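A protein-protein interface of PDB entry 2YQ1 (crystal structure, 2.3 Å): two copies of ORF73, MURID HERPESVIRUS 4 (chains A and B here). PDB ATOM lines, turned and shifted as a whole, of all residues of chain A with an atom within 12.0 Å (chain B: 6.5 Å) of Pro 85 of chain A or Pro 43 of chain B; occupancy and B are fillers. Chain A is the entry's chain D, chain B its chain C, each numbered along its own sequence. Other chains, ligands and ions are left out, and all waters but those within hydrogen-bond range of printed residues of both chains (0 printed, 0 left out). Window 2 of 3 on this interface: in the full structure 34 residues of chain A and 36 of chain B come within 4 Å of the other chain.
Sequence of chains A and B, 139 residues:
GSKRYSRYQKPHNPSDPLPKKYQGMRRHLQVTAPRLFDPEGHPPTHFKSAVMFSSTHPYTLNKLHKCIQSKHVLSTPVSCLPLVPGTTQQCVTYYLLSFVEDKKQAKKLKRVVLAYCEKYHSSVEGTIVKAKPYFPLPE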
ATOM      1  N   LEU A  81      22.256 -10.600  -1.388  1.00  0.00           N
ATOM      2  CA  LEU A  81      22.025 -11.445  -0.233  1.00  0.00           C
ATOM      3  C   LEU A  81      22.071 -12.902  -0.665  1.00  0.00           C
ATOM      4  O   LEU A  81      21.702 -13.231  -1.790  1.00  0.00           O
ATOM      5  CB  LEU A  81      20.682 -11.112   0.411  1.00  0.00           C
ATOM      6  CG  LEU A  81      20.592  -9.679   0.937  1.00  0.00           C
ATOM      7  CD1 LEU A  81      19.202  -9.384   1.451  1.00  0.00           C
ATOM      8  CD2 LEU A  81      21.639  -9.435   2.025  1.00  0.00           C
ATOM      9  N   PRO A  82      22.533 -13.782   0.231  1.00  0.00           N
ATOM     10  CA  PRO A  82      22.582 -15.213  -0.079  1.00  0.00           C
ATOM     11  C   PRO A  82      21.183 -15.805  -0.195  1.00  0.00           C
ATOM     12  O   PRO A  82      20.234 -15.290   0.402  1.00  0.00           O
ATOM     13  CB  PRO A  82      23.304 -15.804   1.135  1.00  0.00           C
ATOM     14  CG  PRO A  82      23.064 -14.813   2.237  1.00  0.00           C
ATOM     15  CD  PRO A  82      23.045 -13.480   1.579  1.00  0.00           C
ATOM     16  N   LEU A  83      21.062 -16.886  -0.956  1.00  0.00           N
ATOM     17  CA  LEU A  83      19.799 -17.593  -1.061  1.00  0.00           C
ATOM     18  C   LEU A  83      19.578 -18.404   0.210  1.00  0.00           C
ATOM     19  O   LEU A  83      20.526 -18.920   0.801  1.00  0.00           O
ATOM     20  CB  LEU A  83      19.786 -18.501  -2.296  1.00  0.00           C
ATOM     21  CG  LEU A  83      20.977 -19.425  -2.579  1.00  0.00           C
ATOM     22  CD1 LEU A  83      20.865 -20.749  -1.822  1.00  0.00           C
ATOM     23  CD2 LEU A  83      21.114 -19.668  -4.076  1.00  0.00           C
ATOM     24  N   VAL A  84      18.326 -18.502   0.634  1.00  0.00           N
ATOM     25  CA  VAL A  84      17.976 -19.342   1.768  1.00  0.00           C
ATOM     26  C   VAL A  84      17.632 -20.727   1.246  1.00  0.00           C
ATOM     27  O   VAL A  84      16.653 -20.883   0.518  1.00  0.00           O
ATOM     28  CB  VAL A  84      16.777 -18.779   2.545  1.00  0.00           C
ATOM     29  CG1 VAL A  84      16.398 -19.717   3.681  1.00  0.00           C
ATOM     30  CG2 VAL A  84      17.094 -17.389   3.077  1.00  0.00           C
ATOM     31  N   PRO A  85      18.464 -21.728   1.591  1.00  0.00           N
ATOM     32  CA  PRO A  85      18.309 -23.115   1.130  1.00  0.00           C
ATOM     33  C   PRO A  85      16.889 -23.613   1.337  1.00  0.00           C
ATOM     34  O   PRO A  85      16.343 -23.469   2.431  1.00  0.00           O
ATOM     35  CB  PRO A  85      19.275 -23.914   2.013  1.00  0.00           C
ATOM     36  CG  PRO A  85      20.045 -22.937   2.812  1.00  0.00           C
ATOM     37  CD  PRO A  85      19.633 -21.547   2.468  1.00  0.00           C
ATOM     38  N   GLY A  86      16.307 -24.194   0.293  1.00  0.00           N
ATOM     39  CA  GLY A  86      14.904 -24.560   0.305  1.00  0.00           C
ATOM     40  C   GLY A  86      14.075 -23.463  -0.335  1.00  0.00           C
ATOM     41  O   GLY A  86      13.182 -22.890   0.286  1.00  0.00           O
ATOM     42  N   THR A  87      14.387 -23.168  -1.593  1.00  0.00           N
ATOM     43  CA  THR A  87      13.686 -22.138  -2.348  1.00  0.00           C
ATOM     44  C   THR A  87      12.364 -22.656  -2.907  1.00  0.00           C
ATOM     45  O   THR A  87      11.810 -22.090  -3.851  1.00  0.00           O
ATOM     46  CB  THR A  87      14.560 -21.607  -3.502  1.00  0.00           C
ATOM     47  OG1 THR A  87      15.301 -22.691  -4.081  1.00  0.00           O
ATOM     48  CG2 THR A  87      15.536 -20.558  -2.990  1.00  0.00           C
ATOM     49  N   CYS A  91      14.539 -15.633  -7.316  1.00  0.00           N
ATOM     50  CA  CYS A  91      15.289 -14.528  -7.910  1.00  0.00           C
ATOM     51  C   CYS A  91      16.182 -13.836  -6.875  1.00  0.00           C
ATOM     52  O   CYS A  91      15.868 -13.826  -5.687  1.00  0.00           O
ATOM     53  CB  CYS A  91      14.345 -13.523  -8.573  1.00  0.00           C
ATOM     54  SG  CYS A  91      13.733 -12.231  -7.478  1.00  0.00           S
ATOM     55  N   THR A  93      17.995 -11.266  -4.462  1.00  0.00           N
ATOM     56  CA  THR A  93      17.727 -10.026  -3.747  1.00  0.00           C
ATOM     57  C   THR A  93      19.033  -9.267  -3.549  1.00  0.00           C
ATOM     58  O   THR A  93      20.013  -9.816  -3.041  1.00  0.00           O
ATOM     59  CB  THR A  93      17.066 -10.281  -2.381  1.00  0.00           C
ATOM     60  OG1 THR A  93      15.830 -10.976  -2.575  1.00  0.00           O
ATOM     61  CG2 THR A  93      16.782  -8.964  -1.675  1.00  0.00           C
ATOM     62  N   PRO B  14      25.104 -23.564  -2.869  1.00  0.00           N
ATOM     63  CA  PRO B  14      25.544 -24.602  -1.930  1.00  0.00           C
ATOM     64  C   PRO B  14      25.955 -25.915  -2.598  1.00  0.00           C
ATOM     65  O   PRO B  14      26.885 -26.567  -2.123  1.00  0.00           O
ATOM     66  CB  PRO B  14      24.308 -24.823  -1.046  1.00  0.00           C
ATOM     67  CG  PRO B  14      23.164 -24.244  -1.812  1.00  0.00           C
ATOM     68  CD  PRO B  14      23.746 -23.090  -2.557  1.00  0.00           C
ATOM     69  N   GLU B  40      22.080 -31.350   8.078  1.00  0.00           N
ATOM     70  CA  GLU B  40      20.718 -31.791   8.317  1.00  0.00           C
ATOM     71  C   GLU B  40      19.886 -30.662   8.900  1.00  0.00           C
ATOM     72  O   GLU B  40      20.413 -29.604   9.253  1.00  0.00           O
ATOM     73  CB  GLU B  40      20.669 -33.025   9.224  1.00  0.00           C
ATOM     74  CG  GLU B  40      21.292 -34.284   8.649  1.00  0.00           C
ATOM     75  CD  GLU B  40      21.210 -35.459   9.612  1.00  0.00           C
ATOM     76  OE1 GLU B  40      20.884 -35.239  10.797  1.00  0.00           O
ATOM     77  OE2 GLU B  40      21.457 -36.604   9.181  1.00  0.00           O
ATOM     78  N   GLY B  41      18.582 -30.886   8.975  1.00  0.00           N
ATOM     79  CA  GLY B  41      17.676 -29.922   9.560  1.00  0.00           C
ATOM     80  C   GLY B  41      17.294 -28.791   8.625  1.00  0.00           C
ATOM     81  O   GLY B  41      17.768 -28.696   7.496  1.00  0.00           O
ATOM     82  N   HIS B  42      16.381 -27.961   9.105  1.00  0.00           N
ATOM     83  CA  HIS B  42      15.936 -26.749   8.431  1.00  0.00           C
ATOM     84  C   HIS B  42      16.681 -25.501   8.895  1.00  0.00           C
ATOM     85  O   HIS B  42      17.020 -25.363  10.069  1.00  0.00           O
ATOM     86  CB  HIS B  42      14.440 -26.551   8.663  1.00  0.00           C
ATOM     87  CG  HIS B  42      13.593 -27.342   7.717  1.00  0.00           C
ATOM     88  ND1 HIS B  42      13.086 -28.586   8.025  1.00  0.00           N
ATOM     89  CD2 HIS B  42      13.203 -27.082   6.445  1.00  0.00           C
ATOM     90  CE1 HIS B  42      12.400 -29.046   6.994  1.00  0.00           C
ATOM     91  NE2 HIS B  42      12.454 -28.152   6.023  1.00  0.00           N
ATOM     92  N   PRO B  43      16.937 -24.588   7.952  1.00  0.00           N
ATOM     93  CA  PRO B  43      17.510 -23.273   8.249  1.00  0.00           C
ATOM     94  C   PRO B  43      16.617 -22.543   9.248  1.00  0.00           C
ATOM     95  O   PRO B  43      15.432 -22.848   9.347  1.00  0.00           O
ATOM     96  CB  PRO B  43      17.507 -22.546   6.896  1.00  0.00           C
ATOM     97  CG  PRO B  43      16.831 -23.438   5.924  1.00  0.00           C
ATOM     98  CD  PRO B  43      16.670 -24.790   6.517  1.00  0.00           C
ATOM     99  N   PRO B  44      17.194 -21.610  10.015  1.00  0.00           N
ATOM    100  CA  PRO B  44      16.414 -20.854  10.999  1.00  0.00           C
ATOM    101  C   PRO B  44      15.350 -20.015  10.317  1.00  0.00           C
ATOM    102  O   PRO B  44      15.505 -19.614   9.164  1.00  0.00           O
ATOM    103  CB  PRO B  44      17.460 -19.951  11.661  1.00  0.00           C
ATOM    104  CG  PRO B  44      18.608 -19.915  10.717  1.00  0.00           C
ATOM    105  CD  PRO B  44      18.618 -21.238  10.028  1.00  0.00           C
ATOM    106  N   THR B  45      14.263 -19.776  11.045  1.00  0.00           N
ATOM    107  CA  THR B  45      13.145 -18.990  10.549  1.00  0.00           C
ATOM    108  C   THR B  45      13.577 -17.570  10.275  1.00  0.00           C
ATOM    109  O   THR B  45      13.209 -17.001   9.247  1.00  0.00           O
ATOM    110  CB  THR B  45      11.985 -18.967  11.561  1.00  0.00           C
ATOM    111  OG1 THR B  45      11.636 -20.310  11.923  1.00  0.00           O
ATOM    112  CG2 THR B  45      10.770 -18.257  10.973  1.00  0.00           C
ATOM    113  N   HIS B  46      14.356 -16.987  11.174  1.00  0.00           N
ATOM    114  CA  HIS B  46      14.830 -15.639  10.921  1.00  0.00           C
ATOM    115  C   HIS B  46      16.323 -15.546  11.180  1.00  0.00           C
ATOM    116  O   HIS B  46      16.864 -16.222  12.051  1.00  0.00           O
ATOM    117  CB  HIS B  46      14.080 -14.624  11.788  1.00  0.00           C
ATOM    118  CG  HIS B  46      12.600 -14.621  11.563  1.00  0.00           C
ATOM    119  ND1 HIS B  46      12.024 -14.158  10.401  1.00  0.00           N
ATOM    120  CD2 HIS B  46      11.580 -15.037  12.350  1.00  0.00           C
ATOM    121  CE1 HIS B  46      10.712 -14.284  10.482  1.00  0.00           C
ATOM    122  NE2 HIS B  46      10.416 -14.813  11.656  1.00  0.00           N
ATOM    123  N   PHE B  47      16.985 -14.707  10.398  1.00  0.00           N
ATOM    124  CA  PHE B  47      18.374 -14.372  10.636  1.00  0.00           C
ATOM    125  C   PHE B  47      18.424 -12.973  11.223  1.00  0.00           C
ATOM    126  O   PHE B  47      18.474 -11.981  10.489  1.00  0.00           O
ATOM    127  CB  PHE B  47      19.174 -14.449   9.339  1.00  0.00           C
ATOM    128  CG  PHE B  47      19.232 -15.835   8.750  1.00  0.00           C
ATOM    129  CD1 PHE B  47      18.160 -16.348   8.031  1.00  0.00           C
ATOM    130  CD2 PHE B  47      20.362 -16.624   8.908  1.00  0.00           C
ATOM    131  CE1 PHE B  47      18.212 -17.623   7.492  1.00  0.00           C
ATOM    132  CE2 PHE B  47      20.418 -17.897   8.367  1.00  0.00           C
ATOM    133  CZ  PHE B  47      19.342 -18.394   7.656  1.00  0.00           C
ATOM    134  N   SER B  70      26.161 -22.868   5.021  1.00  0.00           N
ATOM    135  CA  SER B  70      25.402 -24.057   5.378  1.00  0.00           C
ATOM    136  C   SER B  70      23.932 -23.677   5.399  1.00  0.00           C
ATOM    137  O   SER B  70      23.546 -22.656   4.836  1.00  0.00           O
ATOM    138  CB  SER B  70      25.822 -24.574   6.752  1.00  0.00           C
ATOM    139  OG  SER B  70      25.473 -23.650   7.764  1.00  0.00           O
ATOM    140  N   LYS B  71      23.110 -24.488   6.052  1.00  0.00           N
ATOM    141  CA  LYS B  71      21.703 -24.148   6.200  1.00  0.00           C
ATOM    142  C   LYS B  71      21.508 -23.158   7.331  1.00  0.00           C
ATOM    143  O   LYS B  71      20.475 -22.513   7.429  1.00  0.00           O
ATOM    144  CB  LYS B  71      20.872 -25.399   6.480  1.00  0.00           C
ATOM    145  CG  LYS B  71      20.835 -26.416   5.362  1.00  0.00           C
ATOM    146  CD  LYS B  71      20.087 -27.641   5.836  1.00  0.00           C
ATOM    147  CE  LYS B  71      19.820 -28.630   4.723  1.00  0.00           C
ATOM    148  NZ  LYS B  71      19.161 -29.853   5.272  1.00  0.00           N
ATOM    149  N   HIS B  72      22.521 -23.039   8.180  1.00  0.00           N
ATOM    150  CA  HIS B  72      22.412 -22.265   9.408  1.00  0.00           C
ATOM    151  C   HIS B  72      23.242 -20.988   9.359  1.00  0.00           C
ATOM    152  O   HIS B  72      23.094 -20.102  10.201  1.00  0.00           O
ATOM    153  CB  HIS B  72      22.826 -23.136  10.590  1.00  0.00           C
ATOM    154  CG  HIS B  72      22.313 -24.539  10.485  1.00  0.00           C
ATOM    155  ND1 HIS B  72      21.011 -24.879  10.782  1.00  0.00           N
ATOM    156  CD2 HIS B  72      22.911 -25.677  10.060  1.00  0.00           C
ATOM    157  CE1 HIS B  72      20.838 -26.172  10.571  1.00  0.00           C
ATOM    158  NE2 HIS B  72      21.975 -26.679  10.131  1.00  0.00           N
ATOM    159  N   LEU B  74      24.546 -18.189   6.284  1.00  0.00           N
ATOM    160  CA  LEU B  74      24.549 -17.775   4.891  1.00  0.00           C
ATOM    161  C   LEU B  74      25.450 -16.562   4.707  1.00  0.00           C
ATOM    162  O   LEU B  74      25.286 -15.544   5.385  1.00  0.00           O
ATOM    163  CB  LEU B  74      23.127 -17.451   4.442  1.00  0.00           C
ATOM    164  CG  LEU B  74      22.047 -18.462   4.823  1.00  0.00           C
ATOM    165  CD1 LEU B  74      20.680 -17.975   4.372  1.00  0.00           C
ATOM    166  CD2 LEU B  74      22.365 -19.821   4.239  1.00  0.00           C
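Pro 85 of chain A touches just these residues of chain B: Pro 43, Lys 71 and Leu 74.
No residue of chain A comes within 4 Å of His 42 of chain B.
No residue of chain A comes within 4 Å of Pro 44 of chain B.
No residue of chain A comes within 4 Å of Thr 45 of chain B.
Of the printed residues of chain A, Lys 71 of chain B touches Pro 85.
No residue of chain A comes within 4 Å of His 72 of chain B.
Of the printed residues of chain A, Pro 14 of chain B touches Leu 83 (3.8 Å).
Printed residues of chain B within 4 Å of Pro 82 of chain A: Leu 74.
Printed residues of chain A within 4 Å of Leu 74 of chain B: Pro 82, Leu 83, Val 84 and Pro 85.
Of the printed residues of chain B, Leu 83 of chain A touches Pro 14 and Leu 74.
His 46 of chain B touches none of the printed residues of chain A.
The nearest residue of chain B that does not touch Pro 85 of chain A is Ser 70 of chain B (4.1 Å).
Among the printed residues, merely in contact across the chains: Pro 82 of chain A with Leu 74 of chain B, Leu 83 of chain A with Pro 14 of chain B, Leu 83 of chain A with Leu 74 of chain B, Val 84 of chain A with Leu 74 of chain B, Pro 85 of chain A with Pro 43 of chain B, Pro 85 of chain A with Lys 71 of chain B and Pro 85 of chain A with Leu 74 of chain B.
Hydrophobic or aromatic side chains of chain B within 4 Å of the printed part of chain A: Pro 14, Pro 43 and Leu 74.
Among the printed residues, 7 pairs touch across the chains.
Among the printed residues, no Asp or Glu carboxylate lies within 4 Å of a Lys or Arg side-chain nitrogen of the other chain.
No position is printed for both chains.
The side-chain amino group of Lys 71 of chain B lies within hydrogen-bond range of the backbone carbonyl oxygen of Gly 41 of chain B (2.9 Å).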
